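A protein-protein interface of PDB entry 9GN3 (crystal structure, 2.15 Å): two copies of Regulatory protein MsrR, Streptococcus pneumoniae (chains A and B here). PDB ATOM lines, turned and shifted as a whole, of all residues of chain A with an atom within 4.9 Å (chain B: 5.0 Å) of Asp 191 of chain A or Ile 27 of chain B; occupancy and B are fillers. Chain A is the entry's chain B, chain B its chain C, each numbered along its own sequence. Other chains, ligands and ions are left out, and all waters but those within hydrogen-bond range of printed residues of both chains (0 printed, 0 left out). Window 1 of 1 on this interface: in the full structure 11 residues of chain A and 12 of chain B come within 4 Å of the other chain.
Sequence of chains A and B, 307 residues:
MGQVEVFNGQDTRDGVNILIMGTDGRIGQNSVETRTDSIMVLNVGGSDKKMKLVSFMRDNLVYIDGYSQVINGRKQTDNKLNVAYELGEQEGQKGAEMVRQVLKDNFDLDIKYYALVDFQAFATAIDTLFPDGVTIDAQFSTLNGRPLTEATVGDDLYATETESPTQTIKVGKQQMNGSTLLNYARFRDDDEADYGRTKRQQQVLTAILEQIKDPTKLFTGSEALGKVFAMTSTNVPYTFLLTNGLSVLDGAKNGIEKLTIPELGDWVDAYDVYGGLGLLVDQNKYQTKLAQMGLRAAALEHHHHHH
Of the 11 printed residues of chain A, 4 touch a printed residue of chain B. Printed residues of chain A that touch a printed residue of chain B: Ser 141, Asp 191, Glu 192 and Leu 264. Hydrophobic or aromatic side chains of chain A within 4 Å of the printed part of chain B: Leu 264. Of the 6 printed residues of chain B, 3 touch a printed residue of chain A. Hydrophobic or aromatic side chains of chain B that line the printed part of chain A: Ile 27.
The backbone NH of Leu 143 of chain A is in hydrogen-bond range of the side-chain carboxylate of Asp 191 of chain A (3.5 Å). The side-chain carboxylate of Asp 190 of chain A sits at hydrogen-bond distance from the backbone NH of Glu 192 of chain A, at 2.8 Å. N of Ser 141 of chain A lies within hydrogen-bond range of OD2 of Asp 190 of chain A. The backbone NH (N) of Gly 145 of chain A sits at hydrogen-bond distance from the side-chain carboxylate (OD2) of Asp 191 of chain A, at 3.0 Å. The side-chain amide nitrogen (NE2) of Gln 29 of chain B sits close to the guanidinium group (NH2) of Arg 35 of chain B (3.2 Å). The side-chain carboxylate (OD2) of Asp 191 of chain A lies within hydrogen-bond range of the side-chain hydroxyl (OG1) of Thr 142 of chain A (2.5 Å).
No position is printed for both chains.
OE2 of Glu 192 of chain A lies close to O of Gly 28 of chain B, 2.7 Å away.
Among the printed residues, pairs that only touch across the chains: Ser 141 of chain A with Ile 27 of chain B (3.97 Å), Ser 141 of chain A with Gln 29 of chain B (3.2 Å), Asp 191 of chain A with Ile 27 of chain B (3.1 Å), Glu 192 of chain A with Ile 27 of chain B (3.95 Å), Glu 192 of chain A with Gln 29 of chain B (3.7 Å) and Leu 264 of chain A with Ile 27 of chain B (3.6 Å).
Of the printed residues of chain B, Ser 141 of chain A touches Ile 27 (3.97 Å) and Gln 29 (3.2 Å). Asp 191 of chain A touches one residue of chain B. Of the printed residues of chain B, Leu 264 of chain A touches Ile 27. Gly 25 of chain B touches none of the printed residues of chain A. Ile 27 of chain B touches just these residues of chain A: Ser 141 (3.97 Å), Asp 191 (3.1 Å), Glu 192 (3.95 Å) and Leu 264 (3.6 Å). Of the printed residues of chain A, Gln 29 of chain B touches Ser 141 (3.2 Å) and Glu 192 (3.7 Å). Arg 35 of chain B touches none of the printed residues of chain A. The nearest printed residue of chain B that does not touch Asp 191 of chain A is Gly 25 of chain B (6.7 Å).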
ATOM      1  N   SER A 141      -6.302  -1.643  -2.243  1.00  0.00           N
ATOM      2  CA  SER A 141      -7.206  -2.046  -1.181  1.00  0.00           C
ATOM      3  C   SER A 141      -7.090  -3.560  -0.961  1.00  0.00           C
ATOM      4  O   SER A 141      -6.113  -4.202  -1.363  1.00  0.00           O
ATOM      5  CB  SER A 141      -8.610  -1.647  -1.547  1.00  0.00           C
ATOM      6  OG  SER A 141      -9.478  -1.781  -0.432  1.00  0.00           O
ATOM      7  N   THR A 142      -8.106  -4.138  -0.320  1.00  0.00           N
ATOM      8  CA  THR A 142      -8.191  -5.586  -0.182  1.00  0.00           C
ATOM      9  C   THR A 142      -8.833  -6.148  -1.446  1.00  0.00           C
ATOM     10  O   THR A 142      -9.324  -5.379  -2.269  1.00  0.00           O
ATOM     11  CB  THR A 142      -8.989  -5.965   1.057  1.00  0.00           C
ATOM     12  OG1 THR A 142     -10.198  -5.228   0.933  1.00  0.00           O
ATOM     13  CG2 THR A 142      -8.231  -5.605   2.314  1.00  0.00           C
ATOM     14  N   LEU A 143      -8.794  -7.478  -1.559  1.00  0.00           N
ATOM     15  CA  LEU A 143      -9.589  -8.222  -2.517  1.00  0.00           C
ATOM     16  C   LEU A 143     -10.292  -9.367  -1.793  1.00  0.00           C
ATOM     17  O   LEU A 143      -9.643 -10.309  -1.346  1.00  0.00           O
ATOM     18  CB  LEU A 143      -8.642  -8.748  -3.588  1.00  0.00           C
ATOM     19  CG  LEU A 143      -9.287  -9.416  -4.797  1.00  0.00           C
ATOM     20  CD1 LEU A 143     -10.213  -8.500  -5.585  1.00  0.00           C
ATOM     21  CD2 LEU A 143      -8.158  -9.934  -5.686  1.00  0.00           C
ATOM     22  N   ASN A 144     -11.619  -9.262  -1.670  1.00  0.00           N
ATOM     23  CA  ASN A 144     -12.415 -10.166  -0.855  1.00  0.00           C
ATOM     24  C   ASN A 144     -11.884 -10.221   0.580  1.00  0.00           C
ATOM     25  O   ASN A 144     -11.840 -11.306   1.160  1.00  0.00           O
ATOM     26  CB  ASN A 144     -12.442 -11.563  -1.475  1.00  0.00           C
ATOM     27  CG  ASN A 144     -13.575 -12.413  -0.962  1.00  0.00           C
ATOM     28  OD1 ASN A 144     -13.416 -13.640  -0.802  1.00  0.00           O
ATOM     29  ND2 ASN A 144     -14.733 -11.787  -0.774  1.00  0.00           N
ATOM     30  N   GLY A 145     -11.459  -9.062   1.123  1.00  0.00           N
ATOM     31  CA  GLY A 145     -10.946  -8.955   2.480  1.00  0.00           C
ATOM     32  C   GLY A 145      -9.441  -9.217   2.573  1.00  0.00           C
ATOM     33  O   GLY A 145      -8.800  -8.858   3.549  1.00  0.00           O
ATOM     34  N   ASP A 189      -9.343  -3.267  -9.804  1.00  0.00           N
ATOM     35  CA  ASP A 189      -9.767  -4.647  -9.615  1.00  0.00           C
ATOM     36  C   ASP A 189      -9.496  -5.078  -8.185  1.00  0.00           C
ATOM     37  O   ASP A 189      -8.824  -6.076  -7.961  1.00  0.00           O
ATOM     38  CB  ASP A 189      -9.162  -5.606 -10.630  1.00  0.00           C
ATOM     39  CG  ASP A 189      -9.737  -5.522 -12.035  1.00  0.00           C
ATOM     40  OD1 ASP A 189     -10.983  -5.347 -12.160  1.00  0.00           O
ATOM     41  OD2 ASP A 189      -8.935  -5.668 -12.986  1.00  0.00           O
ATOM     42  N   ASP A 190     -10.048  -4.306  -7.241  1.00  0.00           N
ATOM     43  CA  ASP A 190      -9.952  -4.583  -5.824  1.00  0.00           C
ATOM     44  C   ASP A 190     -11.275  -4.166  -5.189  1.00  0.00           C
ATOM     45  O   ASP A 190     -12.226  -3.812  -5.874  1.00  0.00           O
ATOM     46  CB  ASP A 190      -8.690  -3.992  -5.224  1.00  0.00           C
ATOM     47  CG  ASP A 190      -8.698  -2.499  -4.922  1.00  0.00           C
ATOM     48  OD1 ASP A 190      -9.810  -1.911  -4.837  1.00  0.00           O
ATOM     49  OD2 ASP A 190      -7.581  -1.955  -4.760  1.00  0.00           O
ATOM     50  N   ASP A 191     -11.340  -4.269  -3.867  1.00  0.00           N
ATOM     51  CA  ASP A 191     -12.593  -4.124  -3.140  1.00  0.00           C
ATOM     52  C   ASP A 191     -13.135  -2.697  -3.272  1.00  0.00           C
ATOM     53  O   ASP A 191     -14.336  -2.474  -3.131  1.00  0.00           O
ATOM     54  CB  ASP A 191     -12.421  -4.567  -1.694  1.00  0.00           C
ATOM     55  CG  ASP A 191     -12.367  -6.070  -1.475  1.00  0.00           C
ATOM     56  OD1 ASP A 191     -12.745  -6.840  -2.413  1.00  0.00           O
ATOM     57  OD2 ASP A 191     -11.913  -6.460  -0.378  1.00  0.00           O
ATOM     58  N   GLU A 192     -12.254  -1.736  -3.562  1.00  0.00           N
ATOM     59  CA  GLU A 192     -12.676  -0.351  -3.678  1.00  0.00           C
ATOM     60  C   GLU A 192     -13.145  -0.021  -5.097  1.00  0.00           C
ATOM     61  O   GLU A 192     -13.755   1.026  -5.284  1.00  0.00           O
ATOM     62  CB  GLU A 192     -11.549   0.549  -3.186  1.00  0.00           C
ATOM     63  CG  GLU A 192     -11.441   0.602  -1.665  1.00  0.00           C
ATOM     64  CD  GLU A 192     -10.373   1.581  -1.176  1.00  0.00           C
ATOM     65  OE1 GLU A 192      -9.300   1.779  -1.807  1.00  0.00           O
ATOM     66  OE2 GLU A 192     -10.620   2.141  -0.104  1.00  0.00           O
ATOM     67  N   ALA A 193     -12.864  -0.888  -6.090  1.00  0.00           N
ATOM     68  CA  ALA A 193     -13.372  -0.680  -7.436  1.00  0.00           C
ATOM     69  C   ALA A 193     -13.039   0.746  -7.922  1.00  0.00           C
ATOM     70  O   ALA A 193     -11.908   1.175  -7.711  1.00  0.00           O
ATOM     71  CB  ALA A 193     -14.844  -1.009  -7.448  1.00  0.00           C
ATOM     72  N   LEU A 264     -16.976   6.366  -0.507  1.00  0.00           N
ATOM     73  CA  LEU A 264     -17.119   4.919  -0.577  1.00  0.00           C
ATOM     74  C   LEU A 264     -18.360   4.452   0.179  1.00  0.00           C
ATOM     75  O   LEU A 264     -18.541   4.758   1.341  1.00  0.00           O
ATOM     76  CB  LEU A 264     -15.878   4.218  -0.042  1.00  0.00           C
ATOM     77  CG  LEU A 264     -15.823   2.712  -0.310  1.00  0.00           C
ATOM     78  CD1 LEU A 264     -15.976   2.323  -1.777  1.00  0.00           C
ATOM     79  CD2 LEU A 264     -14.495   2.177   0.207  1.00  0.00           C
ATOM     80  N   GLY B  25     -13.656  -5.271   9.017  1.00  0.00           N
ATOM     81  CA  GLY B  25     -13.931  -5.506   7.610  1.00  0.00           C
ATOM     82  C   GLY B  25     -13.963  -4.190   6.834  1.00  0.00           C
ATOM     83  O   GLY B  25     -13.538  -4.134   5.683  1.00  0.00           O
ATOM     84  N   ARG B  26     -14.485  -3.138   7.471  1.00  0.00           N
ATOM     85  CA  ARG B  26     -14.699  -1.856   6.828  1.00  0.00           C
ATOM     86  C   ARG B  26     -13.821  -1.726   5.582  1.00  0.00           C
ATOM     87  O   ARG B  26     -12.623  -1.418   5.643  1.00  0.00           O
ATOM     88  CB  ARG B  26     -14.533  -0.756   7.872  1.00  0.00           C
ATOM     89  CG  ARG B  26     -15.788  -0.577   8.721  1.00  0.00           C
ATOM     90  CD  ARG B  26     -15.487  -0.168  10.145  1.00  0.00           C
ATOM     91  NE  ARG B  26     -14.363   0.775  10.210  1.00  0.00           N
ATOM     92  CZ  ARG B  26     -13.586   0.963  11.266  1.00  0.00           C
ATOM     93  NH1 ARG B  26     -13.838   0.339  12.398  1.00  0.00           N
ATOM     94  NH2 ARG B  26     -12.548   1.767  11.204  1.00  0.00           N
ATOM     95  N   ILE B  27     -14.488  -1.939   4.433  1.00  0.00           N
ATOM     96  CA  ILE B  27     -13.889  -1.884   3.108  1.00  0.00           C
ATOM     97  C   ILE B  27     -13.057  -0.614   3.026  1.00  0.00           C
ATOM     98  O   ILE B  27     -12.029  -0.600   2.368  1.00  0.00           O
ATOM     99  CB  ILE B  27     -14.976  -1.948   2.014  1.00  0.00           C
ATOM    100  CG1 ILE B  27     -14.405  -2.249   0.634  1.00  0.00           C
ATOM    101  CG2 ILE B  27     -15.850  -0.688   1.998  1.00  0.00           C
ATOM    102  CD1 ILE B  27     -15.428  -2.879  -0.298  1.00  0.00           C
ATOM    103  N   GLY B  28     -13.544   0.417   3.727  1.00  0.00           N
ATOM    104  CA  GLY B  28     -12.903   1.709   3.853  1.00  0.00           C
ATOM    105  C   GLY B  28     -11.444   1.711   3.417  1.00  0.00           C
ATOM    106  O   GLY B  28     -11.100   2.487   2.532  1.00  0.00           O
ATOM    107  N   GLN B  29     -10.604   0.854   4.031  1.00  0.00           N
ATOM    108  CA  GLN B  29      -9.152   0.996   3.989  1.00  0.00           C
ATOM    109  C   GLN B  29      -8.800   2.342   4.627  1.00  0.00           C
ATOM    110  O   GLN B  29      -7.965   2.425   5.521  1.00  0.00           O
ATOM    111  CB  GLN B  29      -8.564   0.771   2.592  1.00  0.00           C
ATOM    112  CG  GLN B  29      -8.200  -0.682   2.311  1.00  0.00           C
ATOM    113  CD  GLN B  29      -6.842  -1.059   2.862  1.00  0.00           C
ATOM    114  OE1 GLN B  29      -5.819  -0.488   2.472  1.00  0.00           O
ATOM    115  NE2 GLN B  29      -6.809  -2.017   3.777  1.00  0.00           N
ATOM    116  N   ARG B  35      -6.298  -4.707  11.180  1.00  0.00           N
ATOM    117  CA  ARG B  35      -7.653  -5.233  11.127  1.00  0.00           C
ATOM    118  C   ARG B  35      -7.986  -6.227  12.242  1.00  0.00           C
ATOM    119  O   ARG B  35      -9.107  -6.689  12.244  1.00  0.00           O
ATOM    120  CB  ARG B  35      -7.951  -5.827   9.751  1.00  0.00           C
ATOM    121  CG  ARG B  35      -7.786  -4.839   8.613  1.00  0.00           C
ATOM    122  CD  ARG B  35      -8.507  -5.286   7.356  1.00  0.00           C
ATOM    123  NE  ARG B  35      -8.608  -4.226   6.346  1.00  0.00           N
ATOM    124  CZ  ARG B  35      -9.707  -3.534   6.006  1.00  0.00           C
ATOM    125  NH1 ARG B  35     -10.796  -3.523   6.759  1.00  0.00           N
ATOM    126  NH2 ARG B  35      -9.708  -2.788   4.914  1.00  0.00           N
